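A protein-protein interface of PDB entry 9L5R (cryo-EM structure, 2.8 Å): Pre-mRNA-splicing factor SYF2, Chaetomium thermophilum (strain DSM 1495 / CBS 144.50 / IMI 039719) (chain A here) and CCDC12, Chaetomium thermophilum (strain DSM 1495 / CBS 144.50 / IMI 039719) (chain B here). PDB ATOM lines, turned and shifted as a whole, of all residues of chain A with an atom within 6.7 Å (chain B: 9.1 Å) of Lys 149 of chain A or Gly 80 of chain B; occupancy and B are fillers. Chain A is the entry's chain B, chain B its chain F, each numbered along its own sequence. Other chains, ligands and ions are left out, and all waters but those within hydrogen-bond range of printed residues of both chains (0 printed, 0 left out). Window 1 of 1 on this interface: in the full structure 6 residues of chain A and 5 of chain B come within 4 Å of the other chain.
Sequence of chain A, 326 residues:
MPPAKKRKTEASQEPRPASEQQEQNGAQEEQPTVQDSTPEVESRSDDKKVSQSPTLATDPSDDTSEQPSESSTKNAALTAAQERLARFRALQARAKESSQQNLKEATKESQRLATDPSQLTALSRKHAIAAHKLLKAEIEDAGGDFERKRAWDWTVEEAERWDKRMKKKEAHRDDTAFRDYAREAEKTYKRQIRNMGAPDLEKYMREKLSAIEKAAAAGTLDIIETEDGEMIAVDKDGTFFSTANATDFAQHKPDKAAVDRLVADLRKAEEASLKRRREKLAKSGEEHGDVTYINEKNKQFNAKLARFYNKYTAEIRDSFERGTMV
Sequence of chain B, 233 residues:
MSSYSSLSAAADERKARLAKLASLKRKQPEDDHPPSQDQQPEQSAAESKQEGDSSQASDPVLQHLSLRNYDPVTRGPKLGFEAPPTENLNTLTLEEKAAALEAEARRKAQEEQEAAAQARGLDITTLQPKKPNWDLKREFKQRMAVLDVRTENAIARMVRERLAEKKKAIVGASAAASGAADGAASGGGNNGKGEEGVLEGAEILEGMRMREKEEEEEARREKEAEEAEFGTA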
ATOM      1  N   ILE A 139       3.526  -7.406 -22.834  1.00  0.00           N
ATOM      2  CA  ILE A 139       3.775  -8.358 -21.749  1.00  0.00           C
ATOM      3  C   ILE A 139       3.844  -7.645 -20.400  1.00  0.00           C
ATOM      4  O   ILE A 139       3.135  -8.014 -19.455  1.00  0.00           O
ATOM      5  CB  ILE A 139       5.032  -9.197 -22.023  1.00  0.00           C
ATOM      6  CG1 ILE A 139       4.747 -10.201 -23.134  1.00  0.00           C
ATOM      7  CG2 ILE A 139       5.451  -9.938 -20.777  1.00  0.00           C
ATOM      8  CD1 ILE A 139       3.648 -11.162 -22.799  1.00  0.00           C
ATOM      9  N   GLY A 144       2.816  -9.699 -16.922  1.00  0.00           N
ATOM     10  CA  GLY A 144       3.748 -10.802 -16.877  1.00  0.00           C
ATOM     11  C   GLY A 144       5.188 -10.337 -16.951  1.00  0.00           C
ATOM     12  O   GLY A 144       5.502  -9.232 -17.391  1.00  0.00           O
ATOM     13  N   ASP A 145       6.086 -11.207 -16.503  1.00  0.00           N
ATOM     14  CA  ASP A 145       7.512 -10.915 -16.523  1.00  0.00           C
ATOM     15  C   ASP A 145       8.078 -11.408 -17.847  1.00  0.00           C
ATOM     16  O   ASP A 145       8.146 -12.618 -18.093  1.00  0.00           O
ATOM     17  CB  ASP A 145       8.216 -11.559 -15.335  1.00  0.00           C
ATOM     18  CG  ASP A 145       9.629 -11.044 -15.146  1.00  0.00           C
ATOM     19  OD1 ASP A 145      10.510 -11.399 -15.957  1.00  0.00           O
ATOM     20  OD2 ASP A 145       9.855 -10.275 -14.188  1.00  0.00           O
ATOM     21  N   PHE A 146       8.477 -10.461 -18.696  1.00  0.00           N
ATOM     22  CA  PHE A 146       9.012 -10.793 -20.010  1.00  0.00           C
ATOM     23  C   PHE A 146      10.297 -11.598 -19.891  1.00  0.00           C
ATOM     24  O   PHE A 146      10.526 -12.541 -20.660  1.00  0.00           O
ATOM     25  CB  PHE A 146       9.239  -9.505 -20.793  1.00  0.00           C
ATOM     26  CG  PHE A 146       9.792  -9.705 -22.163  1.00  0.00           C
ATOM     27  CD1 PHE A 146       9.056 -10.348 -23.135  1.00  0.00           C
ATOM     28  CD2 PHE A 146      11.037  -9.211 -22.491  1.00  0.00           C
ATOM     29  CE1 PHE A 146       9.565 -10.516 -24.405  1.00  0.00           C
ATOM     30  CE2 PHE A 146      11.547  -9.373 -23.756  1.00  0.00           C
ATOM     31  CZ  PHE A 146      10.811 -10.026 -24.714  1.00  0.00           C
ATOM     32  N   GLU A 147      11.128 -11.275 -18.906  1.00  0.00           N
ATOM     33  CA  GLU A 147      12.378 -12.001 -18.769  1.00  0.00           C
ATOM     34  C   GLU A 147      12.184 -13.390 -18.185  1.00  0.00           C
ATOM     35  O   GLU A 147      12.943 -14.295 -18.524  1.00  0.00           O
ATOM     36  CB  GLU A 147      13.371 -11.192 -17.944  1.00  0.00           C
ATOM     37  CG  GLU A 147      13.915 -10.006 -18.712  1.00  0.00           C
ATOM     38  CD  GLU A 147      14.574 -10.403 -20.028  1.00  0.00           C
ATOM     39  OE1 GLU A 147      15.240 -11.455 -20.085  1.00  0.00           O
ATOM     40  OE2 GLU A 147      14.423  -9.658 -21.016  1.00  0.00           O
ATOM     41  N   ARG A 148      11.164 -13.605 -17.354  1.00  0.00           N
ATOM     42  CA  ARG A 148      10.842 -14.965 -16.931  1.00  0.00           C
ATOM     43  C   ARG A 148      10.250 -15.795 -18.065  1.00  0.00           C
ATOM     44  O   ARG A 148      10.606 -16.978 -18.234  1.00  0.00           O
ATOM     45  CB  ARG A 148       9.875 -14.912 -15.753  1.00  0.00           C
ATOM     46  CG  ARG A 148      10.510 -14.402 -14.479  1.00  0.00           C
ATOM     47  CD  ARG A 148       9.528 -14.390 -13.329  1.00  0.00           C
ATOM     48  NE  ARG A 148       9.272 -15.727 -12.811  1.00  0.00           N
ATOM     49  CZ  ARG A 148       8.411 -15.998 -11.841  1.00  0.00           C
ATOM     50  NH1 ARG A 148       7.700 -15.047 -11.261  1.00  0.00           N
ATOM     51  NH2 ARG A 148       8.258 -17.257 -11.446  1.00  0.00           N
ATOM     52  N   LYS A 149       9.378 -15.191 -18.864  1.00  0.00           N
ATOM     53  CA  LYS A 149       8.826 -15.864 -20.025  1.00  0.00           C
ATOM     54  C   LYS A 149       9.894 -16.211 -21.058  1.00  0.00           C
ATOM     55  O   LYS A 149       9.750 -17.197 -21.784  1.00  0.00           O
ATOM     56  CB  LYS A 149       7.740 -14.993 -20.650  1.00  0.00           C
ATOM     57  CG  LYS A 149       6.476 -14.916 -19.820  1.00  0.00           C
ATOM     58  CD  LYS A 149       5.494 -13.929 -20.405  1.00  0.00           C
ATOM     59  CE  LYS A 149       4.955 -14.441 -21.718  1.00  0.00           C
ATOM     60  NZ  LYS A 149       3.842 -15.403 -21.504  1.00  0.00           N
ATOM     61  N   ARG A 150      10.964 -15.420 -21.145  1.00  0.00           N
ATOM     62  CA  ARG A 150      12.087 -15.791 -22.002  1.00  0.00           C
ATOM     63  C   ARG A 150      13.030 -16.769 -21.305  1.00  0.00           C
ATOM     64  O   ARG A 150      13.730 -17.559 -21.970  1.00  0.00           O
ATOM     65  CB  ARG A 150      12.834 -14.532 -22.421  1.00  0.00           C
ATOM     66  CG  ARG A 150      12.064 -13.651 -23.367  1.00  0.00           C
ATOM     67  CD  ARG A 150      12.989 -12.998 -24.358  1.00  0.00           C
ATOM     68  NE  ARG A 150      13.882 -12.048 -23.712  1.00  0.00           N
ATOM     69  CZ  ARG A 150      14.725 -11.259 -24.359  1.00  0.00           C
ATOM     70  NH1 ARG A 150      14.838 -11.302 -25.674  1.00  0.00           N
ATOM     71  NH2 ARG A 150      15.471 -10.405 -23.670  1.00  0.00           N
ATOM     72  N   ALA A 151      13.054 -16.726 -19.969  1.00  0.00           N
ATOM     73  CA  ALA A 151      13.860 -17.643 -19.178  1.00  0.00           C
ATOM     74  C   ALA A 151      13.403 -19.066 -19.382  1.00  0.00           C
ATOM     75  O   ALA A 151      14.187 -20.009 -19.244  1.00  0.00           O
ATOM     76  CB  ALA A 151      13.788 -17.270 -17.701  1.00  0.00           C
ATOM     77  N   TRP A 152      12.142 -19.240 -19.744  1.00  0.00           N
ATOM     78  CA  TRP A 152      11.723 -20.579 -20.145  1.00  0.00           C
ATOM     79  C   TRP A 152      12.363 -21.050 -21.452  1.00  0.00           C
ATOM     80  O   TRP A 152      12.243 -22.227 -21.793  1.00  0.00           O
ATOM     81  CB  TRP A 152      10.201 -20.670 -20.254  1.00  0.00           C
ATOM     82  CG  TRP A 152       9.559 -20.905 -18.939  1.00  0.00           C
ATOM     83  CD1 TRP A 152       8.683 -20.084 -18.305  1.00  0.00           C
ATOM     84  CD2 TRP A 152       9.766 -22.020 -18.068  1.00  0.00           C
ATOM     85  NE1 TRP A 152       8.318 -20.622 -17.101  1.00  0.00           N
ATOM     86  CE2 TRP A 152       8.971 -21.813 -16.934  1.00  0.00           C
ATOM     87  CE3 TRP A 152      10.538 -23.181 -18.143  1.00  0.00           C
ATOM     88  CZ2 TRP A 152       8.928 -22.716 -15.884  1.00  0.00           C
ATOM     89  CZ3 TRP A 152      10.497 -24.069 -17.100  1.00  0.00           C
ATOM     90  CH2 TRP A 152       9.698 -23.837 -15.988  1.00  0.00           C
ATOM     91  N   ASP A 153      13.048 -20.169 -22.196  1.00  0.00           N
ATOM     92  CA  ASP A 153      13.542 -20.573 -23.509  1.00  0.00           C
ATOM     93  C   ASP A 153      15.038 -20.369 -23.739  1.00  0.00           C
ATOM     94  O   ASP A 153      15.529 -20.741 -24.808  1.00  0.00           O
ATOM     95  CB  ASP A 153      12.803 -19.835 -24.616  1.00  0.00           C
ATOM     96  CG  ASP A 153      11.435 -20.393 -24.860  1.00  0.00           C
ATOM     97  OD1 ASP A 153      11.258 -21.609 -24.666  1.00  0.00           O
ATOM     98  OD2 ASP A 153      10.543 -19.620 -25.256  1.00  0.00           O
ATOM     99  N   TRP A 154      15.780 -19.774 -22.807  1.00  0.00           N
ATOM    100  CA  TRP A 154      17.232 -19.655 -22.988  1.00  0.00           C
ATOM    101  C   TRP A 154      17.930 -21.013 -22.924  1.00  0.00           C
ATOM    102  O   TRP A 154      17.620 -21.828 -22.056  1.00  0.00           O
ATOM    103  CB  TRP A 154      17.852 -18.734 -21.941  1.00  0.00           C
ATOM    104  CG  TRP A 154      17.268 -17.381 -21.884  1.00  0.00           C
ATOM    105  CD1 TRP A 154      16.717 -16.792 -20.802  1.00  0.00           C
ATOM    106  CD2 TRP A 154      17.173 -16.434 -22.949  1.00  0.00           C
ATOM    107  NE1 TRP A 154      16.278 -15.539 -21.113  1.00  0.00           N
ATOM    108  CE2 TRP A 154      16.549 -15.295 -22.432  1.00  0.00           C
ATOM    109  CE3 TRP A 154      17.563 -16.438 -24.286  1.00  0.00           C
ATOM    110  CZ2 TRP A 154      16.302 -14.175 -23.199  1.00  0.00           C
ATOM    111  CZ3 TRP A 154      17.310 -15.334 -25.043  1.00  0.00           C
ATOM    112  CH2 TRP A 154      16.686 -14.216 -24.503  1.00  0.00           C
ATOM    113  N   ARG B  68       5.638 -33.477 -27.096  1.00  0.00           N
ATOM    114  CA  ARG B  68       6.058 -32.809 -25.874  1.00  0.00           C
ATOM    115  C   ARG B  68       7.009 -31.653 -26.134  1.00  0.00           C
ATOM    116  O   ARG B  68       6.820 -30.567 -25.584  1.00  0.00           O
ATOM    117  CB  ARG B  68       6.717 -33.809 -24.923  1.00  0.00           C
ATOM    118  CG  ARG B  68       7.200 -33.191 -23.640  1.00  0.00           C
ATOM    119  CD  ARG B  68       7.488 -34.251 -22.611  1.00  0.00           C
ATOM    120  NE  ARG B  68       6.259 -34.736 -22.002  1.00  0.00           N
ATOM    121  CZ  ARG B  68       6.174 -35.838 -21.274  1.00  0.00           C
ATOM    122  NH1 ARG B  68       7.229 -36.598 -21.050  1.00  0.00           N
ATOM    123  NH2 ARG B  68       4.998 -36.188 -20.764  1.00  0.00           N
ATOM    124  N   ASN B  69       8.026 -31.859 -26.964  1.00  0.00           N
ATOM    125  CA  ASN B  69       8.943 -30.793 -27.333  1.00  0.00           C
ATOM    126  C   ASN B  69       8.685 -30.248 -28.725  1.00  0.00           C
ATOM    127  O   ASN B  69       9.040 -29.100 -29.003  1.00  0.00           O
ATOM    128  CB  ASN B  69      10.391 -31.288 -27.253  1.00  0.00           C
ATOM    129  CG  ASN B  69      10.733 -31.855 -25.898  1.00  0.00           C
ATOM    130  OD1 ASN B  69      10.945 -31.117 -24.939  1.00  0.00           O
ATOM    131  ND2 ASN B  69      10.779 -33.174 -25.806  1.00  0.00           N
ATOM    132  N   PRO B  77      10.448 -26.586 -32.570  1.00  0.00           N
ATOM    133  CA  PRO B  77      10.319 -26.868 -31.138  1.00  0.00           C
ATOM    134  C   PRO B  77       9.235 -26.027 -30.483  1.00  0.00           C
ATOM    135  O   PRO B  77       8.905 -24.930 -30.935  1.00  0.00           O
ATOM    136  CB  PRO B  77      11.700 -26.511 -30.585  1.00  0.00           C
ATOM    137  CG  PRO B  77      12.211 -25.494 -31.531  1.00  0.00           C
ATOM    138  CD  PRO B  77      11.709 -25.897 -32.881  1.00  0.00           C
ATOM    139  N   LYS B  78       8.683 -26.563 -29.402  1.00  0.00           N
ATOM    140  CA  LYS B  78       7.670 -25.853 -28.639  1.00  0.00           C
ATOM    141  C   LYS B  78       8.326 -24.834 -27.718  1.00  0.00           C
ATOM    142  O   LYS B  78       9.315 -25.131 -27.046  1.00  0.00           O
ATOM    143  CB  LYS B  78       6.830 -26.835 -27.826  1.00  0.00           C
ATOM    144  CG  LYS B  78       5.512 -26.267 -27.347  1.00  0.00           C
ATOM    145  CD  LYS B  78       4.552 -27.372 -26.941  1.00  0.00           C
ATOM    146  CE  LYS B  78       4.863 -27.894 -25.553  1.00  0.00           C
ATOM    147  NZ  LYS B  78       3.867 -28.905 -25.112  1.00  0.00           N
ATOM    148  N   LEU B  79       7.764 -23.631 -27.687  1.00  0.00           N
ATOM    149  CA  LEU B  79       8.342 -22.514 -26.955  1.00  0.00           C
ATOM    150  C   LEU B  79       7.685 -22.378 -25.590  1.00  0.00           C
ATOM    151  O   LEU B  79       6.456 -22.400 -25.483  1.00  0.00           O
ATOM    152  CB  LEU B  79       8.177 -21.213 -27.736  1.00  0.00           C
ATOM    153  CG  LEU B  79       8.994 -21.085 -29.014  1.00  0.00           C
ATOM    154  CD1 LEU B  79       8.742 -19.741 -29.659  1.00  0.00           C
ATOM    155  CD2 LEU B  79      10.464 -21.266 -28.710  1.00  0.00           C
ATOM    156  N   GLY B  80       8.505 -22.228 -24.553  1.00  0.00           N
ATOM    157  CA  GLY B  80       7.998 -21.916 -23.232  1.00  0.00           C
ATOM    158  C   GLY B  80       7.613 -20.471 -23.033  1.00  0.00           C
ATOM    159  O   GLY B  80       7.066 -20.125 -21.982  1.00  0.00           O
ATOM    160  N   PHE B  81       7.908 -19.617 -24.012  1.00  0.00           N
ATOM    161  CA  PHE B  81       7.462 -18.233 -23.952  1.00  0.00           C
ATOM    162  C   PHE B  81       5.950 -18.143 -24.078  1.00  0.00           C
ATOM    163  O   PHE B  81       5.312 -17.316 -23.420  1.00  0.00           O
ATOM    164  CB  PHE B  81       8.138 -17.421 -25.053  1.00  0.00           C
ATOM    165  CG  PHE B  81       7.755 -15.977 -25.063  1.00  0.00           C
ATOM    166  CD1 PHE B  81       8.266 -15.111 -24.122  1.00  0.00           C
ATOM    167  CD2 PHE B  81       6.885 -15.487 -26.013  1.00  0.00           C
ATOM    168  CE1 PHE B  81       7.916 -13.782 -24.122  1.00  0.00           C
ATOM    169  CE2 PHE B  81       6.531 -14.160 -26.016  1.00  0.00           C
ATOM    170  CZ  PHE B  81       7.050 -13.306 -25.069  1.00  0.00           C
ATOM    171  N   GLU B  82       5.364 -18.990 -24.921  1.00  0.00           N
ATOM    172  CA  GLU B  82       3.928 -18.983 -25.164  1.00  0.00           C
ATOM    173  C   GLU B  82       3.191 -19.953 -24.251  1.00  0.00           C
ATOM    174  O   GLU B  82       2.222 -19.573 -23.589  1.00  0.00           O
ATOM    175  CB  GLU B  82       3.650 -19.324 -26.627  1.00  0.00           C
ATOM    176  CG  GLU B  82       4.426 -18.472 -27.606  1.00  0.00           C
ATOM    177  CD  GLU B  82       4.709 -19.197 -28.899  1.00  0.00           C
ATOM    178  OE1 GLU B  82       4.143 -20.291 -29.103  1.00  0.00           O
ATOM    179  OE2 GLU B  82       5.493 -18.670 -29.715  1.00  0.00           O
ATOM    180  N   ALA B  83       3.639 -21.202 -24.200  1.00  0.00           N
ATOM    181  CA  ALA B  83       2.989 -22.234 -23.394  1.00  0.00           C
ATOM    182  C   ALA B  83       3.953 -22.729 -22.331  1.00  0.00           C
ATOM    183  O   ALA B  83       4.744 -23.653 -22.590  1.00  0.00           O
ATOM    184  CB  ALA B  83       2.519 -23.390 -24.272  1.00  0.00           C
ATOM    185  N   PRO B  84       3.938 -22.145 -21.133  1.00  0.00           N
ATOM    186  CA  PRO B  84       4.785 -22.656 -20.063  1.00  0.00           C
ATOM    187  C   PRO B  84       4.317 -24.028 -19.618  1.00  0.00           C
ATOM    188  O   PRO B  84       3.125 -24.359 -19.737  1.00  0.00           O
ATOM    189  CB  PRO B  84       4.606 -21.617 -18.941  1.00  0.00           C
ATOM    190  CG  PRO B  84       4.045 -20.418 -19.603  1.00  0.00           C
ATOM    191  CD  PRO B  84       3.229 -20.919 -20.741  1.00  0.00           C
ATOM    192  N   PRO B  85       5.217 -24.866 -19.103  1.00  0.00           N
ATOM    193  CA  PRO B  85       4.796 -26.125 -18.481  1.00  0.00           C
ATOM    194  C   PRO B  85       4.006 -25.952 -17.193  1.00  0.00           C
ATOM    195  O   PRO B  85       3.342 -26.901 -16.762  1.00  0.00           O
ATOM    196  CB  PRO B  85       6.126 -26.843 -18.213  1.00  0.00           C
ATOM    197  CG  PRO B  85       7.163 -25.809 -18.245  1.00  0.00           C
ATOM    198  CD  PRO B  85       6.670 -24.652 -19.038  1.00  0.00           C
ATOM    199  N   THR B  86       4.053 -24.770 -16.581  1.00  0.00           N
ATOM    200  CA  THR B  86       3.180 -24.445 -15.465  1.00  0.00           C
ATOM    201  C   THR B  86       1.707 -24.467 -15.843  1.00  0.00           C
ATOM    202  O   THR B  86       0.863 -24.695 -14.970  1.00  0.00           O
ATOM    203  CB  THR B  86       3.539 -23.070 -14.897  1.00  0.00           C
ATOM    204  OG1 THR B  86       3.224 -22.059 -15.860  1.00  0.00           O
ATOM    205  CG2 THR B  86       5.017 -23.002 -14.572  1.00  0.00           C
ATOM    206  N   GLU B  87       1.378 -24.229 -17.117  1.00  0.00           N
ATOM    207  CA  GLU B  87       0.020 -24.480 -17.586  1.00  0.00           C
ATOM    208  C   GLU B  87      -0.309 -25.966 -17.535  1.00  0.00           C
ATOM    209  O   GLU B  87      -1.378 -26.357 -17.053  1.00  0.00           O
ATOM    210  CB  GLU B  87      -0.153 -23.956 -19.009  1.00  0.00           C
ATOM    211  CG  GLU B  87      -0.003 -22.458 -19.158  1.00  0.00           C
ATOM    212  CD  GLU B  87      -0.434 -21.975 -20.529  1.00  0.00           C
ATOM    213  OE1 GLU B  87      -0.984 -22.791 -21.297  1.00  0.00           O
ATOM    214  OE2 GLU B  87      -0.225 -20.784 -20.841  1.00  0.00           O
ATOM    215  N   ASN B  88       0.608 -26.806 -18.014  1.00  0.00           N
ATOM    216  CA  ASN B  88       0.384 -28.244 -18.069  1.00  0.00           C
ATOM    217  C   ASN B  88       0.437 -28.912 -16.701  1.00  0.00           C
ATOM    218  O   ASN B  88       0.058 -30.082 -16.597  1.00  0.00           O
ATOM    219  CB  ASN B  88       1.412 -28.894 -18.996  1.00  0.00           C
ATOM    220  CG  ASN B  88       1.281 -28.425 -20.432  1.00  0.00           C
ATOM    221  OD1 ASN B  88       2.175 -27.771 -20.967  1.00  0.00           O
ATOM    222  ND2 ASN B  88       0.164 -28.760 -21.065  1.00  0.00           N
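Of the 14 printed residues of chain B, 4 touch a printed residue of chain A. Printed residues of chain B that touch a printed residue of chain A: Leu 79, Gly 80, Phe 81 and Pro 85. Hydrophobic or aromatic side chains of chain B that line the printed part of chain A: Leu 79, Phe 81 and Pro 85. Hydrophobic or aromatic side chains of chain A within 4 Å of the printed part of chain B: Phe 146 and Trp 152. Among the printed residues, no Asp or Glu carboxylate lies within 4 Å of a Lys or Arg side-chain nitrogen of the other chain.
Of chain B, only Gly 80 and Phe 81 come within 4 Å of Lys 149 of chain A. Of the printed residues of chain A, Gly 80 of chain B touches Lys 149, Trp 152 and Asp 153. Of the printed residues of chain A, Leu 79 of chain B touches Asp 153. Of the printed residues of chain B, Trp 152 of chain A touches Gly 80 and Pro 85. Printed residues of chain B within 4 Å of Phe 146 of chain A: Phe 81 (3.7 Å). Glu 87 of chain B touches none of the printed residues of chain A. The nearest residue of chain B that does not touch Lys 149 of chain A is Glu 82 of chain B (4.9 Å). The nearest printed residue of chain A that does not touch Leu 79 of chain B is Trp 152 of chain A (5.9 Å).
Phe 146 of chain A touches Phe 81 of chain B. Lys 149 of chain A touches Gly 80 of chain B. Gly 80 of chain B touches Trp 152 of chain A. Pro 85 of chain B touches Trp 152 of chain A. Leu 79 of chain B touches Asp 153 of chain A.
O of Phe 81 of chain B is in hydrogen-bond range of NZ of Lys 149 of chain A (3.1 Å). OD1 of Asp 153 of chain A lies within hydrogen-bond range of N of Gly 80 of chain B (2.8 Å). The backbone NH (N) of Phe 81 of chain B lies within hydrogen-bond range of the side-chain carboxylate (OD2) of Asp 153 of chain A, at 2.9 Å.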
